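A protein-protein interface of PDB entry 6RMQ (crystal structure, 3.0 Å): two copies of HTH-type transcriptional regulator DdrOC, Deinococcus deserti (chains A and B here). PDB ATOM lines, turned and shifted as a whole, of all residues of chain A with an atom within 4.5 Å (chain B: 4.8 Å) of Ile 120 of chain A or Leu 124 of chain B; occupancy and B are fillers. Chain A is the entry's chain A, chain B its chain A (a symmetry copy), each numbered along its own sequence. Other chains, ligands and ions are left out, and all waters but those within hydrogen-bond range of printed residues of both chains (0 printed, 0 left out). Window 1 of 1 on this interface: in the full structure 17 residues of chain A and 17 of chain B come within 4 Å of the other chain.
Printed residues of chain A that touch a printed residue of chain B: Pro 111, Asp 116, Glu 119, Ile 120, His 123 and Leu 124.
Hydrophobic or aromatic side chains of chain A within 4 Å of the printed part of chain B: Pro 111, Ile 120, His 123 and Leu 124.
Printed residues of chain B that touch a printed residue of chain A: Ile 120, His 123, Leu 124, Ile 127 and Leu 128.
Hydrophobic or aromatic side chains of chain B within 4 Å of the printed part of chain A: Ile 120, His 123, Leu 124, Ile 127 and Leu 128.
Among the printed residues, 7 pairs touch across the chains.
Pro 111 of chain A touches Leu 128 of chain B.
Asp 116 of chain A touches Ile 127 of chain B (OD2 to CG2, 3.7 Å).
Ile 120 of chain A touches Leu 124 of chain B (CD1 to CD2, 3.8 Å).
Ile 127 of chain B touches Ile 120 of chain A.
Leu 124 of chain A touches Ile 120 of chain B.
The side-chain carboxylate (OE2) of Glu 119 of chain A lies within hydrogen-bond range of a ring nitrogen (NE2) of His 123 of chain B (2.7 Å).
ND1 of His 123 of chain A is in hydrogen-bond range of ND1 of His 123 of chain B.
Printed residues of chain B within 4 Å of Glu 119 of chain A: His 123.
Leu 122 of chain B touches none of the printed residues of chain A.
Leu 124 of chain B touches one residue of chain A.
Of the printed residues of chain A, Ile 127 of chain B touches Asp 116 (3.7 Å) and Ile 120 (3.6 Å).
The nearest printed residue of chain B that does not touch Ile 120 of chain A is His 123 of chain B (5.1 Å).
The indole nitrogen (NE1) of Trp 117 of chain A lies within hydrogen-bond range of the backbone carbonyl oxygen (O) of Pro 111 of chain A.
Ile 120 of chain A touches Leu 124 of chain B, and with the chains exchanged Leu 124 of chain A touches Ile 120 of chain B.
His 123 of chain B touches its own counterpart, His 123 of chain A.
Of the 7 pairs that touch across the chains among the printed residues, 3 have their exchanged pair printed and touching as well.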
ATOM      1  N   ILE A 104      -2.206  35.878  21.044  1.00  0.00           N
ATOM      2  CA  ILE A 104      -2.277  34.560  21.658  1.00  0.00           C
ATOM      3  C   ILE A 104      -1.846  34.681  23.126  1.00  0.00           C
ATOM      4  O   ILE A 104      -0.684  35.002  23.434  1.00  0.00           O
ATOM      5  CB  ILE A 104      -1.458  33.498  20.887  1.00  0.00           C
ATOM      6  CG1 ILE A 104      -1.963  33.375  19.448  1.00  0.00           C
ATOM      7  CG2 ILE A 104      -1.600  32.142  21.552  1.00  0.00           C
ATOM      8  CD1 ILE A 104      -0.966  32.785  18.462  1.00  0.00           C
ATOM      9  N   PRO A 111       3.322  31.749  25.321  1.00  0.00           N
ATOM     10  CA  PRO A 111       4.513  30.954  25.082  1.00  0.00           C
ATOM     11  C   PRO A 111       5.781  31.671  25.610  1.00  0.00           C
ATOM     12  O   PRO A 111       5.874  32.908  25.565  1.00  0.00           O
ATOM     13  CB  PRO A 111       4.534  30.819  23.561  1.00  0.00           C
ATOM     14  CG  PRO A 111       3.155  31.157  23.109  1.00  0.00           C
ATOM     15  CD  PRO A 111       2.642  32.141  24.079  1.00  0.00           C
ATOM     16  N   ASP A 116       9.114  28.048  21.218  1.00  0.00           N
ATOM     17  CA  ASP A 116       7.699  28.056  21.587  1.00  0.00           C
ATOM     18  C   ASP A 116       6.834  28.851  20.563  1.00  0.00           C
ATOM     19  O   ASP A 116       5.816  28.364  20.073  1.00  0.00           O
ATOM     20  CB  ASP A 116       7.516  28.654  22.984  1.00  0.00           C
ATOM     21  CG  ASP A 116       8.023  27.748  24.122  1.00  0.00           C
ATOM     22  OD1 ASP A 116       9.258  27.633  24.331  1.00  0.00           O
ATOM     23  OD2 ASP A 116       7.160  27.207  24.858  1.00  0.00           O
ATOM     24  N   TRP A 117       7.271  30.062  20.224  1.00  0.00           N
ATOM     25  CA  TRP A 117       6.560  30.953  19.296  1.00  0.00           C
ATOM     26  C   TRP A 117       6.607  30.465  17.870  1.00  0.00           C
ATOM     27  O   TRP A 117       5.624  30.563  17.124  1.00  0.00           O
ATOM     28  CB  TRP A 117       7.122  32.376  19.373  1.00  0.00           C
ATOM     29  CG  TRP A 117       6.703  33.091  20.620  1.00  0.00           C
ATOM     30  CD1 TRP A 117       7.431  33.243  21.773  1.00  0.00           C
ATOM     31  CD2 TRP A 117       5.422  33.699  20.871  1.00  0.00           C
ATOM     32  NE1 TRP A 117       6.688  33.924  22.719  1.00  0.00           N
ATOM     33  CE2 TRP A 117       5.457  34.221  22.190  1.00  0.00           C
ATOM     34  CE3 TRP A 117       4.245  33.844  20.115  1.00  0.00           C
ATOM     35  CZ2 TRP A 117       4.373  34.883  22.754  1.00  0.00           C
ATOM     36  CZ3 TRP A 117       3.169  34.518  20.680  1.00  0.00           C
ATOM     37  CH2 TRP A 117       3.242  35.025  21.984  1.00  0.00           C
ATOM     38  N   TYR A 118       7.756  29.927  17.497  1.00  0.00           N
ATOM     39  CA  TYR A 118       7.951  29.440  16.150  1.00  0.00           C
ATOM     40  C   TYR A 118       7.137  28.162  15.914  1.00  0.00           C
ATOM     41  O   TYR A 118       6.675  27.902  14.789  1.00  0.00           O
ATOM     42  CB  TYR A 118       9.452  29.240  15.878  1.00  0.00           C
ATOM     43  CG  TYR A 118       9.779  29.119  14.414  1.00  0.00           C
ATOM     44  CD1 TYR A 118       9.191  29.979  13.491  1.00  0.00           C
ATOM     45  CD2 TYR A 118      10.676  28.135  13.947  1.00  0.00           C
ATOM     46  CE1 TYR A 118       9.467  29.872  12.146  1.00  0.00           C
ATOM     47  CE2 TYR A 118      10.962  28.016  12.586  1.00  0.00           C
ATOM     48  CZ  TYR A 118      10.346  28.892  11.688  1.00  0.00           C
ATOM     49  OH  TYR A 118      10.574  28.832  10.323  1.00  0.00           O
ATOM     50  N   GLU A 119       6.949  27.395  16.994  1.00  0.00           N
ATOM     51  CA  GLU A 119       6.193  26.156  16.980  1.00  0.00           C
ATOM     52  C   GLU A 119       4.799  26.470  16.498  1.00  0.00           C
ATOM     53  O   GLU A 119       4.296  25.826  15.583  1.00  0.00           O
ATOM     54  CB  GLU A 119       6.155  25.544  18.384  1.00  0.00           C
ATOM     55  CG  GLU A 119       5.803  24.052  18.421  1.00  0.00           C
ATOM     56  CD  GLU A 119       5.766  23.451  19.835  1.00  0.00           C
ATOM     57  OE1 GLU A 119       6.437  24.023  20.736  1.00  0.00           O
ATOM     58  OE2 GLU A 119       5.069  22.410  20.040  1.00  0.00           O
ATOM     59  N   ILE A 120       4.211  27.498  17.101  1.00  0.00           N
ATOM     60  CA  ILE A 120       2.842  27.892  16.841  1.00  0.00           C
ATOM     61  C   ILE A 120       2.747  28.489  15.475  1.00  0.00           C
ATOM     62  O   ILE A 120       1.838  28.133  14.710  1.00  0.00           O
ATOM     63  CB  ILE A 120       2.362  28.994  17.774  1.00  0.00           C
ATOM     64  CG1 ILE A 120       2.524  28.605  19.221  1.00  0.00           C
ATOM     65  CG2 ILE A 120       0.896  29.288  17.501  1.00  0.00           C
ATOM     66  CD1 ILE A 120       2.059  29.697  20.150  1.00  0.00           C
ATOM     67  N   TYR A 121       3.652  29.426  15.183  1.00  0.00           N
ATOM     68  CA  TYR A 121       3.607  30.134  13.915  1.00  0.00           C
ATOM     69  C   TYR A 121       3.470  29.137  12.765  1.00  0.00           C
ATOM     70  O   TYR A 121       2.573  29.293  11.918  1.00  0.00           O
ATOM     71  CB  TYR A 121       4.808  31.049  13.723  1.00  0.00           C
ATOM     72  CG  TYR A 121       5.019  31.384  12.283  1.00  0.00           C
ATOM     73  CD1 TYR A 121       4.243  32.362  11.651  1.00  0.00           C
ATOM     74  CD2 TYR A 121       5.970  30.693  11.520  1.00  0.00           C
ATOM     75  CE1 TYR A 121       4.415  32.665  10.297  1.00  0.00           C
ATOM     76  CE2 TYR A 121       6.147  30.984  10.171  1.00  0.00           C
ATOM     77  CZ  TYR A 121       5.367  31.971   9.569  1.00  0.00           C
ATOM     78  OH  TYR A 121       5.532  32.243   8.242  1.00  0.00           O
ATOM     79  N   LEU A 122       4.319  28.103  12.780  1.00  0.00           N
ATOM     80  CA  LEU A 122       4.364  27.108  11.718  1.00  0.00           C
ATOM     81  C   LEU A 122       3.084  26.290  11.619  1.00  0.00           C
ATOM     82  O   LEU A 122       2.566  26.074  10.502  1.00  0.00           O
ATOM     83  CB  LEU A 122       5.541  26.178  11.905  1.00  0.00           C
ATOM     84  CG  LEU A 122       6.921  26.774  11.674  1.00  0.00           C
ATOM     85  CD1 LEU A 122       7.944  25.926  12.412  1.00  0.00           C
ATOM     86  CD2 LEU A 122       7.244  26.924  10.188  1.00  0.00           C
ATOM     87  N   HIS A 123       2.569  25.829  12.770  1.00  0.00           N
ATOM     88  CA  HIS A 123       1.299  25.111  12.787  1.00  0.00           C
ATOM     89  C   HIS A 123       0.213  26.008  12.188  1.00  0.00           C
ATOM     90  O   HIS A 123      -0.425  25.596  11.216  1.00  0.00           O
ATOM     91  CB  HIS A 123       0.929  24.613  14.185  1.00  0.00           C
ATOM     92  CG  HIS A 123      -0.074  23.490  14.188  1.00  0.00           C
ATOM     93  ND1 HIS A 123      -0.328  22.721  15.312  1.00  0.00           N
ATOM     94  CD2 HIS A 123      -0.862  22.986  13.196  1.00  0.00           C
ATOM     95  CE1 HIS A 123      -1.247  21.811  15.013  1.00  0.00           C
ATOM     96  NE2 HIS A 123      -1.585  21.951  13.738  1.00  0.00           N
ATOM     97  N   LEU A 124       0.058  27.238  12.706  1.00  0.00           N
ATOM     98  CA  LEU A 124      -1.037  28.125  12.267  1.00  0.00           C
ATOM     99  C   LEU A 124      -0.881  28.547  10.835  1.00  0.00           C
ATOM    100  O   LEU A 124      -1.875  28.694  10.118  1.00  0.00           O
ATOM    101  CB  LEU A 124      -1.140  29.396  13.099  1.00  0.00           C
ATOM    102  CG  LEU A 124      -1.499  29.326  14.564  1.00  0.00           C
ATOM    103  CD1 LEU A 124      -1.528  30.763  15.051  1.00  0.00           C
ATOM    104  CD2 LEU A 124      -2.824  28.598  14.806  1.00  0.00           C
ATOM    105  N   TRP B  97     -10.765  29.636  27.335  1.00  0.00           N
ATOM    106  CA  TRP B  97     -10.103  29.128  26.128  1.00  0.00           C
ATOM    107  C   TRP B  97     -10.814  29.543  24.867  1.00  0.00           C
ATOM    108  O   TRP B  97     -10.194  29.798  23.829  1.00  0.00           O
ATOM    109  CB  TRP B  97      -9.986  27.613  26.164  1.00  0.00           C
ATOM    110  CG  TRP B  97      -8.673  27.157  26.710  1.00  0.00           C
ATOM    111  CD1 TRP B  97      -8.430  26.630  27.948  1.00  0.00           C
ATOM    112  CD2 TRP B  97      -7.406  27.219  26.049  1.00  0.00           C
ATOM    113  NE1 TRP B  97      -7.099  26.343  28.092  1.00  0.00           N
ATOM    114  CE2 TRP B  97      -6.446  26.691  26.942  1.00  0.00           C
ATOM    115  CE3 TRP B  97      -6.988  27.654  24.779  1.00  0.00           C
ATOM    116  CZ2 TRP B  97      -5.084  26.603  26.613  1.00  0.00           C
ATOM    117  CZ3 TRP B  97      -5.644  27.563  24.446  1.00  0.00           C
ATOM    118  CH2 TRP B  97      -4.704  27.045  25.361  1.00  0.00           C
ATOM    119  N   LEU B 101      -9.229  31.464  21.883  1.00  0.00           N
ATOM    120  CA  LEU B 101      -9.291  30.953  20.511  1.00  0.00           C
ATOM    121  C   LEU B 101      -9.990  31.858  19.491  1.00  0.00           C
ATOM    122  O   LEU B 101      -9.751  31.729  18.281  1.00  0.00           O
ATOM    123  CB  LEU B 101      -9.947  29.568  20.476  1.00  0.00           C
ATOM    124  CG  LEU B 101      -9.349  28.367  21.198  1.00  0.00           C
ATOM    125  CD1 LEU B 101     -10.431  27.321  21.112  1.00  0.00           C
ATOM    126  CD2 LEU B 101      -8.023  27.889  20.613  1.00  0.00           C
ATOM    127  N   ILE B 104      -7.791  34.318  17.220  1.00  0.00           N
ATOM    128  CA  ILE B 104      -6.916  33.775  16.192  1.00  0.00           C
ATOM    129  C   ILE B 104      -7.530  34.077  14.818  1.00  0.00           C
ATOM    130  O   ILE B 104      -8.613  33.575  14.470  1.00  0.00           O
ATOM    131  CB  ILE B 104      -6.626  32.268  16.391  1.00  0.00           C
ATOM    132  CG1 ILE B 104      -5.964  32.026  17.749  1.00  0.00           C
ATOM    133  CG2 ILE B 104      -5.683  31.769  15.313  1.00  0.00           C
ATOM    134  CD1 ILE B 104      -6.094  30.610  18.288  1.00  0.00           C
ATOM    135  N   ILE B 120      -5.804  23.234  16.830  1.00  0.00           N
ATOM    136  CA  ILE B 120      -5.084  24.341  17.423  1.00  0.00           C
ATOM    137  C   ILE B 120      -5.222  24.283  18.910  1.00  0.00           C
ATOM    138  O   ILE B 120      -4.219  24.423  19.626  1.00  0.00           O
ATOM    139  CB  ILE B 120      -5.663  25.694  17.037  1.00  0.00           C
ATOM    140  CG1 ILE B 120      -5.730  25.861  15.541  1.00  0.00           C
ATOM    141  CG2 ILE B 120      -4.803  26.801  17.622  1.00  0.00           C
ATOM    142  CD1 ILE B 120      -6.312  27.196  15.152  1.00  0.00           C
ATOM    143  N   TYR B 121      -6.463  24.125  19.375  1.00  0.00           N
ATOM    144  CA  TYR B 121      -6.729  24.137  20.803  1.00  0.00           C
ATOM    145  C   TYR B 121      -5.758  23.203  21.523  1.00  0.00           C
ATOM    146  O   TYR B 121      -5.108  23.620  22.498  1.00  0.00           O
ATOM    147  CB  TYR B 121      -8.177  23.795  21.123  1.00  0.00           C
ATOM    148  CG  TYR B 121      -8.334  23.335  22.536  1.00  0.00           C
ATOM    149  CD1 TYR B 121      -8.377  24.255  23.590  1.00  0.00           C
ATOM    150  CD2 TYR B 121      -8.397  21.969  22.840  1.00  0.00           C
ATOM    151  CE1 TYR B 121      -8.499  23.834  24.918  1.00  0.00           C
ATOM    152  CE2 TYR B 121      -8.514  21.540  24.159  1.00  0.00           C
ATOM    153  CZ  TYR B 121      -8.565  22.478  25.189  1.00  0.00           C
ATOM    154  OH  TYR B 121      -8.664  22.052  26.482  1.00  0.00           O
ATOM    155  N   LEU B 122      -5.630  21.976  21.005  1.00  0.00           N
ATOM    156  CA  LEU B 122      -4.802  20.947  21.617  1.00  0.00           C
ATOM    157  C   LEU B 122      -3.321  21.300  21.612  1.00  0.00           C
ATOM    158  O   LEU B 122      -2.635  21.125  22.642  1.00  0.00           O
ATOM    159  CB  LEU B 122      -5.003  19.617  20.926  1.00  0.00           C
ATOM    160  CG  LEU B 122      -6.347  18.938  21.139  1.00  0.00           C
ATOM    161  CD1 LEU B 122      -6.584  17.965  19.995  1.00  0.00           C
ATOM    162  CD2 LEU B 122      -6.446  18.270  22.509  1.00  0.00           C
ATOM    163  N   HIS B 123      -2.819  21.789  20.467  1.00  0.00           N
ATOM    164  CA  HIS B 123      -1.433  22.239  20.391  1.00  0.00           C
ATOM    165  C   HIS B 123      -1.207  23.336  21.433  1.00  0.00           C
ATOM    166  O   HIS B 123      -0.323  23.177  22.278  1.00  0.00           O
ATOM    167  CB  HIS B 123      -1.043  22.693  18.982  1.00  0.00           C
ATOM    168  CG  HIS B 123       0.441  22.700  18.731  1.00  0.00           C
ATOM    169  ND1 HIS B 123       0.981  22.807  17.459  1.00  0.00           N
ATOM    170  CD2 HIS B 123       1.498  22.582  19.585  1.00  0.00           C
ATOM    171  CE1 HIS B 123       2.305  22.780  17.550  1.00  0.00           C
ATOM    172  NE2 HIS B 123       2.642  22.643  18.826  1.00  0.00           N
ATOM    173  N   LEU B 124      -2.039  24.392  21.424  1.00  0.00           N
ATOM    174  CA  LEU B 124      -1.826  25.547  22.318  1.00  0.00           C
ATOM    175  C   LEU B 124      -2.006  25.182  23.763  1.00  0.00           C
ATOM    176  O   LEU B 124      -1.303  25.709  24.630  1.00  0.00           O
ATOM    177  CB  LEU B 124      -2.771  26.704  22.027  1.00  0.00           C
ATOM    178  CG  LEU B 124      -2.700  27.440  20.710  1.00  0.00           C
ATOM    179  CD1 LEU B 124      -3.758  28.524  20.784  1.00  0.00           C
ATOM    180  CD2 LEU B 124      -1.303  28.002  20.431  1.00  0.00           C
ATOM    181  N   LYS B 125      -2.965  24.288  24.009  1.00  0.00           N
ATOM    182  CA  LYS B 125      -3.229  23.798  25.344  1.00  0.00           C
ATOM    183  C   LYS B 125      -1.923  23.314  25.961  1.00  0.00           C
ATOM    184  O   LYS B 125      -1.597  23.738  27.055  1.00  0.00           O
ATOM    185  CB  LYS B 125      -4.352  22.745  25.342  1.00  0.00           C
ATOM    186  CG  LYS B 125      -5.118  22.646  26.660  1.00  0.00           C
ATOM    187  CD  LYS B 125      -4.598  21.450  27.459  1.00  0.00           C
ATOM    188  CE  LYS B 125      -4.345  21.745  28.933  1.00  0.00           C
ATOM    189  NZ  LYS B 125      -5.629  21.911  29.673  1.00  0.00           N
ATOM    190  N   ARG B 126      -1.151  22.513  25.219  1.00  0.00           N
ATOM    191  CA  ARG B 126       0.179  22.067  25.650  1.00  0.00           C
ATOM    192  C   ARG B 126       1.108  23.214  25.926  1.00  0.00           C
ATOM    193  O   ARG B 126       1.745  23.224  26.977  1.00  0.00           O
ATOM    194  CB  ARG B 126       0.879  21.191  24.619  1.00  0.00           C
ATOM    195  CG  ARG B 126       0.346  19.787  24.505  1.00  0.00           C
ATOM    196  CD  ARG B 126       1.444  18.834  24.066  1.00  0.00           C
ATOM    197  NE  ARG B 126       1.319  17.605  24.835  1.00  0.00           N
ATOM    198  CZ  ARG B 126       0.404  16.655  24.617  1.00  0.00           C
ATOM    199  NH1 ARG B 126      -0.474  16.747  23.625  1.00  0.00           N
ATOM    200  NH2 ARG B 126       0.373  15.586  25.400  1.00  0.00           N
ATOM    201  N   ILE B 127       1.189  24.169  24.985  1.00  0.00           N
ATOM    202  CA  ILE B 127       2.159  25.266  25.084  1.00  0.00           C
ATOM    203  C   ILE B 127       1.820  26.195  26.263  1.00  0.00           C
ATOM    204  O   ILE B 127       2.704  26.598  27.017  1.00  0.00           O
ATOM    205  CB  ILE B 127       2.375  26.004  23.745  1.00  0.00           C
ATOM    206  CG1 ILE B 127       2.714  25.017  22.634  1.00  0.00           C
ATOM    207  CG2 ILE B 127       3.577  26.919  23.840  1.00  0.00           C
ATOM    208  CD1 ILE B 127       2.579  25.575  21.242  1.00  0.00           C
ATOM    209  N   LEU B 128       0.545  26.483  26.476  1.00  0.00           N
ATOM    210  CA  LEU B 128       0.147  27.308  27.623  1.00  0.00           C
ATOM    211  C   LEU B 128      -0.511  26.418  28.679  1.00  0.00           C
ATOM    212  O   LEU B 128      -1.173  26.903  29.600  1.00  0.00           O
ATOM    213  CB  LEU B 128      -0.762  28.482  27.187  1.00  0.00           C
ATOM    214  CG  LEU B 128      -0.751  28.970  25.714  1.00  0.00           C
ATOM    215  CD1 LEU B 128      -2.021  29.696  25.312  1.00  0.00           C
ATOM    216  CD2 LEU B 128       0.439  29.837  25.411  1.00  0.00           C
